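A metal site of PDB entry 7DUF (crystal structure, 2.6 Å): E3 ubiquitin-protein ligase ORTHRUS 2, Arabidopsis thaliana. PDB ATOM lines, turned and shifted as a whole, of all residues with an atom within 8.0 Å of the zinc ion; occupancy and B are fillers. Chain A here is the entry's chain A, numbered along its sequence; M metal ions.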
ATOM      1  N   MET A   5       7.748 -13.438 -15.685  1.00  0.00           N
ATOM      2  CA  MET A   5       8.041 -14.841 -15.935  1.00  0.00           C
ATOM      3  C   MET A   5       7.219 -15.404 -17.085  1.00  0.00           C
ATOM      4  O   MET A   5       7.772 -16.052 -17.992  1.00  0.00           O
ATOM      5  CB  MET A   5       7.780 -15.652 -14.660  1.00  0.00           C
ATOM      6  CG  MET A   5       8.964 -15.758 -13.718  1.00  0.00           C
ATOM      7  SD  MET A   5      10.012 -17.181 -14.079  1.00  0.00           S
ATOM      8  CE  MET A   5       8.771 -18.474 -14.213  1.00  0.00           C
ATOM      9  N   LEU A  11      -1.589 -17.013 -14.729  1.00  0.00           N
ATOM     10  CA  LEU A  11      -2.540 -17.602 -13.805  1.00  0.00           C
ATOM     11  C   LEU A  11      -2.540 -16.841 -12.482  1.00  0.00           C
ATOM     12  O   LEU A  11      -1.473 -16.393 -12.024  1.00  0.00           O
ATOM     13  CB  LEU A  11      -2.227 -19.081 -13.545  1.00  0.00           C
ATOM     14  CG  LEU A  11      -2.801 -20.067 -14.560  1.00  0.00           C
ATOM     15  CD1 LEU A  11      -1.903 -20.162 -15.783  1.00  0.00           C
ATOM     16  CD2 LEU A  11      -2.998 -21.448 -13.939  1.00  0.00           C
ATOM     17  N   PRO A  12      -3.698 -16.666 -11.844  1.00  0.00           N
ATOM     18  CA  PRO A  12      -3.741 -15.930 -10.571  1.00  0.00           C
ATOM     19  C   PRO A  12      -3.357 -16.795  -9.375  1.00  0.00           C
ATOM     20  O   PRO A  12      -2.679 -17.816  -9.533  1.00  0.00           O
ATOM     21  CB  PRO A  12      -5.206 -15.480 -10.494  1.00  0.00           C
ATOM     22  CG  PRO A  12      -5.950 -16.587 -11.179  1.00  0.00           C
ATOM     23  CD  PRO A  12      -5.039 -17.105 -12.276  1.00  0.00           C
ATOM     24  N   CYS A  13      -3.780 -16.388  -8.193  1.00  0.00           N
ATOM     25  CA  CYS A  13      -3.486 -17.116  -6.967  1.00  0.00           C
ATOM     26  C   CYS A  13      -4.672 -17.962  -6.534  1.00  0.00           C
ATOM     27  O   CYS A  13      -5.768 -17.907  -7.109  1.00  0.00           O
ATOM     28  CB  CYS A  13      -3.061 -16.166  -5.848  1.00  0.00           C
ATOM     29  SG  CYS A  13      -1.296 -15.772  -5.832  1.00  0.00           S
ATOM     30  N   VAL A  18      -1.833 -19.552  -2.892  1.00  0.00           N
ATOM     31  CA  VAL A  18      -0.835 -20.295  -3.660  1.00  0.00           C
ATOM     32  C   VAL A  18      -0.935 -19.874  -5.120  1.00  0.00           C
ATOM     33  O   VAL A  18      -2.032 -19.798  -5.681  1.00  0.00           O
ATOM     34  CB  VAL A  18      -1.028 -21.817  -3.514  1.00  0.00           C
ATOM     35  CG1 VAL A  18       0.105 -22.559  -4.222  1.00  0.00           C
ATOM     36  CG2 VAL A  18      -1.086 -22.198  -2.048  1.00  0.00           C
ATOM     37  N   CYS A  19       0.220 -19.601  -5.740  1.00  0.00           N
ATOM     38  CA  CYS A  19       0.243 -19.258  -7.153  1.00  0.00           C
ATOM     39  C   CYS A  19      -0.096 -20.488  -7.986  1.00  0.00           C
ATOM     40  O   CYS A  19       0.563 -21.526  -7.879  1.00  0.00           O
ATOM     41  CB  CYS A  19       1.625 -18.725  -7.544  1.00  0.00           C
ATOM     42  SG  CYS A  19       1.767 -18.216  -9.278  1.00  0.00           S
ATOM     43  N   MET A  20      -1.138 -20.362  -8.821  1.00  0.00           N
ATOM     44  CA  MET A  20      -1.564 -21.478  -9.646  1.00  0.00           C
ATOM     45  C   MET A  20      -0.506 -21.884 -10.671  1.00  0.00           C
ATOM     46  O   MET A  20      -0.590 -22.990 -11.217  1.00  0.00           O
ATOM     47  CB  MET A  20      -2.871 -21.134 -10.363  1.00  0.00           C
ATOM     48  CG  MET A  20      -4.038 -20.845  -9.436  1.00  0.00           C
ATOM     49  SD  MET A  20      -5.622 -21.128 -10.253  1.00  0.00           S
ATOM     50  CE  MET A  20      -6.621 -19.823  -9.546  1.00  0.00           C
ATOM     51  N   ARG A  21       0.468 -21.018 -10.943  1.00  0.00           N
ATOM     52  CA  ARG A  21       1.462 -21.277 -11.970  1.00  0.00           C
ATOM     53  C   ARG A  21       2.732 -21.907 -11.404  1.00  0.00           C
ATOM     54  O   ARG A  21       3.191 -22.940 -11.910  1.00  0.00           O
ATOM     55  CB  ARG A  21       1.803 -19.980 -12.712  1.00  0.00           C
ATOM     56  CG  ARG A  21       2.582 -20.188 -14.003  1.00  0.00           C
ATOM     57  CD  ARG A  21       2.633 -18.906 -14.820  1.00  0.00           C
ATOM     58  NE  ARG A  21       3.397 -19.082 -16.050  1.00  0.00           N
ATOM     59  CZ  ARG A  21       4.719 -18.994 -16.132  1.00  0.00           C
ATOM     60  NH1 ARG A  21       5.459 -18.728 -15.069  1.00  0.00           N
ATOM     61  NH2 ARG A  21       5.304 -19.184 -17.303  1.00  0.00           N
ATOM     62  N   CYS A  22       3.310 -21.314 -10.363  1.00  0.00           N
ATOM     63  CA  CYS A  22       4.591 -21.768  -9.833  1.00  0.00           C
ATOM     64  C   CYS A  22       4.463 -22.568  -8.534  1.00  0.00           C
ATOM     65  O   CYS A  22       5.490 -22.961  -7.975  1.00  0.00           O
ATOM     66  CB  CYS A  22       5.529 -20.571  -9.613  1.00  0.00           C
ATOM     67  SG  CYS A  22       5.136 -19.555  -8.171  1.00  0.00           S
ATOM     68  N   LYS A  23       3.240 -22.802  -8.057  1.00  0.00           N
ATOM     69  CA  LYS A  23       2.996 -23.678  -6.906  1.00  0.00           C
ATOM     70  C   LYS A  23       3.682 -23.164  -5.645  1.00  0.00           C
ATOM     71  O   LYS A  23       4.155 -23.949  -4.817  1.00  0.00           O
ATOM     72  CB  LYS A  23       3.415 -25.113  -7.202  1.00  0.00           C
ATOM     73  CG  LYS A  23       2.599 -25.801  -8.281  1.00  0.00           C
ATOM     74  CD  LYS A  23       1.217 -26.153  -7.776  1.00  0.00           C
ATOM     75  CE  LYS A  23       0.165 -25.825  -8.812  1.00  0.00           C
ATOM     76  NZ  LYS A  23      -1.104 -25.458  -8.146  1.00  0.00           N
ATOM     77  N   SER A  24       3.745 -21.848  -5.499  1.00  0.00           N
ATOM     78  CA  SER A  24       4.365 -21.224  -4.334  1.00  0.00           C
ATOM     79  C   SER A  24       3.377 -20.287  -3.652  1.00  0.00           C
ATOM     80  O   SER A  24       2.406 -19.833  -4.261  1.00  0.00           O
ATOM     81  CB  SER A  24       5.637 -20.459  -4.713  1.00  0.00           C
ATOM     82  OG  SER A  24       5.895 -19.407  -3.797  1.00  0.00           O
ATOM     83  N   ASN A  25       3.641 -20.012  -2.373  1.00  0.00           N
ATOM     84  CA  ASN A  25       2.851 -19.049  -1.622  1.00  0.00           C
ATOM     85  C   ASN A  25       3.607 -17.729  -1.594  1.00  0.00           C
ATOM     86  O   ASN A  25       4.553 -17.579  -0.806  1.00  0.00           O
ATOM     87  CB  ASN A  25       2.598 -19.558  -0.195  1.00  0.00           C
ATOM     88  CG  ASN A  25       1.434 -18.851   0.480  1.00  0.00           C
ATOM     89  OD1 ASN A  25       1.239 -17.646   0.311  1.00  0.00           O
ATOM     90  ND2 ASN A  25       0.647 -19.603   1.241  1.00  0.00           N
ATOM     91  N   PRO A  26       3.253 -16.757  -2.416  1.00  0.00           N
ATOM     92  CA  PRO A  26       4.050 -15.536  -2.539  1.00  0.00           C
ATOM     93  C   PRO A  26       4.013 -14.716  -1.265  1.00  0.00           C
ATOM     94  O   PRO A  26       2.945 -14.542  -0.659  1.00  0.00           O
ATOM     95  CB  PRO A  26       3.376 -14.778  -3.696  1.00  0.00           C
ATOM     96  CG  PRO A  26       2.612 -15.834  -4.448  1.00  0.00           C
ATOM     97  CD  PRO A  26       2.144 -16.773  -3.387  1.00  0.00           C
ATOM     98  N   GLU A  30       5.750  -9.862  -2.906  1.00  0.00           N
ATOM     99  CA  GLU A  30       5.587 -10.429  -4.240  1.00  0.00           C
ATOM    100  C   GLU A  30       4.118 -10.594  -4.624  1.00  0.00           C
ATOM    101  O   GLU A  30       3.827 -11.252  -5.625  1.00  0.00           O
ATOM    102  CB  GLU A  30       6.302 -11.779  -4.338  1.00  0.00           C
ATOM    103  CG  GLU A  30       7.761 -11.764  -3.929  1.00  0.00           C
ATOM    104  CD  GLU A  30       8.509 -12.990  -4.407  1.00  0.00           C
ATOM    105  OE1 GLU A  30       9.657 -13.196  -3.961  1.00  0.00           O
ATOM    106  OE2 GLU A  30       7.954 -13.735  -5.234  1.00  0.00           O
ATOM    107  N   TRP A  41      -2.462 -11.796  -7.389  1.00  0.00           N
ATOM    108  CA  TRP A  41      -1.613 -12.339  -8.440  1.00  0.00           C
ATOM    109  C   TRP A  41      -0.169 -12.352  -7.967  1.00  0.00           C
ATOM    110  O   TRP A  41       0.263 -11.450  -7.241  1.00  0.00           O
ATOM    111  CB  TRP A  41      -1.714 -11.508  -9.727  1.00  0.00           C
ATOM    112  CG  TRP A  41      -3.046 -11.613 -10.409  1.00  0.00           C
ATOM    113  CD1 TRP A  41      -4.228 -11.085  -9.980  1.00  0.00           C
ATOM    114  CD2 TRP A  41      -3.328 -12.280 -11.643  1.00  0.00           C
ATOM    115  NE1 TRP A  41      -5.226 -11.384 -10.867  1.00  0.00           N
ATOM    116  CE2 TRP A  41      -4.707 -12.120 -11.906  1.00  0.00           C
ATOM    117  CE3 TRP A  41      -2.561 -13.001 -12.558  1.00  0.00           C
ATOM    118  CZ2 TRP A  41      -5.324 -12.646 -13.034  1.00  0.00           C
ATOM    119  CZ3 TRP A  41      -3.171 -13.534 -13.682  1.00  0.00           C
ATOM    120  CH2 TRP A  41      -4.540 -13.346 -13.912  1.00  0.00           C
ATOM    121  N   HIS A  42       0.561 -13.385  -8.362  1.00  0.00           N
ATOM    122  CA  HIS A  42       1.993 -13.461  -8.072  1.00  0.00           C
ATOM    123  C   HIS A  42       2.736 -12.567  -9.058  1.00  0.00           C
ATOM    124  O   HIS A  42       2.783 -12.863 -10.256  1.00  0.00           O
ATOM    125  CB  HIS A  42       2.485 -14.909  -8.159  1.00  0.00           C
ATOM    126  CG  HIS A  42       3.875 -15.097  -7.656  1.00  0.00           C
ATOM    127  ND1 HIS A  42       4.599 -16.248  -7.886  1.00  0.00           N
ATOM    128  CD2 HIS A  42       4.695 -14.280  -6.943  1.00  0.00           C
ATOM    129  CE1 HIS A  42       5.797 -16.134  -7.332  1.00  0.00           C
ATOM    130  NE2 HIS A  42       5.870 -14.946  -6.755  1.00  0.00           N
ATOM    131  N   VAL A  43       3.304 -11.463  -8.556  1.00  0.00           N
ATOM    132  CA  VAL A  43       3.891 -10.458  -9.433  1.00  0.00           C
ATOM    133  C   VAL A  43       5.081 -11.018 -10.195  1.00  0.00           C
ATOM    134  O   VAL A  43       5.417 -10.530 -11.278  1.00  0.00           O
ATOM    135  CB  VAL A  43       4.270  -9.202  -8.626  1.00  0.00           C
ATOM    136  CG1 VAL A  43       5.659  -9.343  -8.001  1.00  0.00           C
ATOM    137  CG2 VAL A  43       4.193  -7.959  -9.498  1.00  0.00           C
ATOM    138  N   SER A  44       5.736 -12.051  -9.668  1.00  0.00           N
ATOM    139  CA  SER A  44       6.866 -12.648 -10.357  1.00  0.00           C
ATOM    140  C   SER A  44       6.417 -13.367 -11.626  1.00  0.00           C
ATOM    141  O   SER A  44       7.097 -13.308 -12.656  1.00  0.00           O
ATOM    142  CB  SER A  44       7.613 -13.608  -9.436  1.00  0.00           C
ATOM    143  OG  SER A  44       8.143 -14.699 -10.159  1.00  0.00           O
ATOM    144  N   CYS A  45       5.271 -14.036 -11.572  1.00  0.00           N
ATOM    145  CA  CYS A  45       4.780 -14.848 -12.678  1.00  0.00           C
ATOM    146  C   CYS A  45       3.945 -14.055 -13.686  1.00  0.00           C
ATOM    147  O   CYS A  45       3.285 -14.662 -14.538  1.00  0.00           O
ATOM    148  CB  CYS A  45       3.952 -16.022 -12.145  1.00  0.00           C
ATOM    149  SG  CYS A  45       4.913 -17.277 -11.273  1.00  0.00           S
ATOM    150  N   LEU A  46       3.967 -12.725 -13.605  1.00  0.00           N
ATOM    151  CA  LEU A  46       3.209 -11.927 -14.551  1.00  0.00           C
ATOM    152  C   LEU A  46       3.962 -11.812 -15.876  1.00  0.00           C
ATOM    153  O   LEU A  46       5.158 -12.088 -15.970  1.00  0.00           O
ATOM    154  CB  LEU A  46       2.947 -10.522 -13.983  1.00  0.00           C
ATOM    155  CG  LEU A  46       1.793 -10.397 -12.989  1.00  0.00           C
ATOM    156  CD1 LEU A  46       1.645  -8.963 -12.527  1.00  0.00           C
ATOM    157  CD2 LEU A  46       0.491 -10.897 -13.609  1.00  0.00           C
HETATM  158 ZN    ZN M   1       4.041 -17.777  -9.181  1.00  0.00          ZN
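The nearest printed residue that does not touch the zinc ion is Arg 21 (4.7 Å).
SG of Cys 22 lies close to N of Ser 24 (3.8 Å). The backbone NH (N) of Cys 19 sits at hydrogen-bond distance from the backbone carbonyl oxygen (O) of Ser 24, at 2.6 Å. SG of Cys 19 sits close to N of Arg 21 (3.5 Å). A ring nitrogen (NE2) of His 42 sits at hydrogen-bond distance from the side-chain carboxylate (OE2) of Glu 30, at 2.9 Å.
The zinc ion is bound by a ring nitrogen (ND1) of His 42 (2.1 Å), the side-chain sulfur of Cys 22 (2.3 Å), the side-chain sulfur of Cys 19 (2.3 Å) and the side-chain sulfur of Cys 45 (2.3 Å). The zinc ion has four donor atoms within binding distance.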
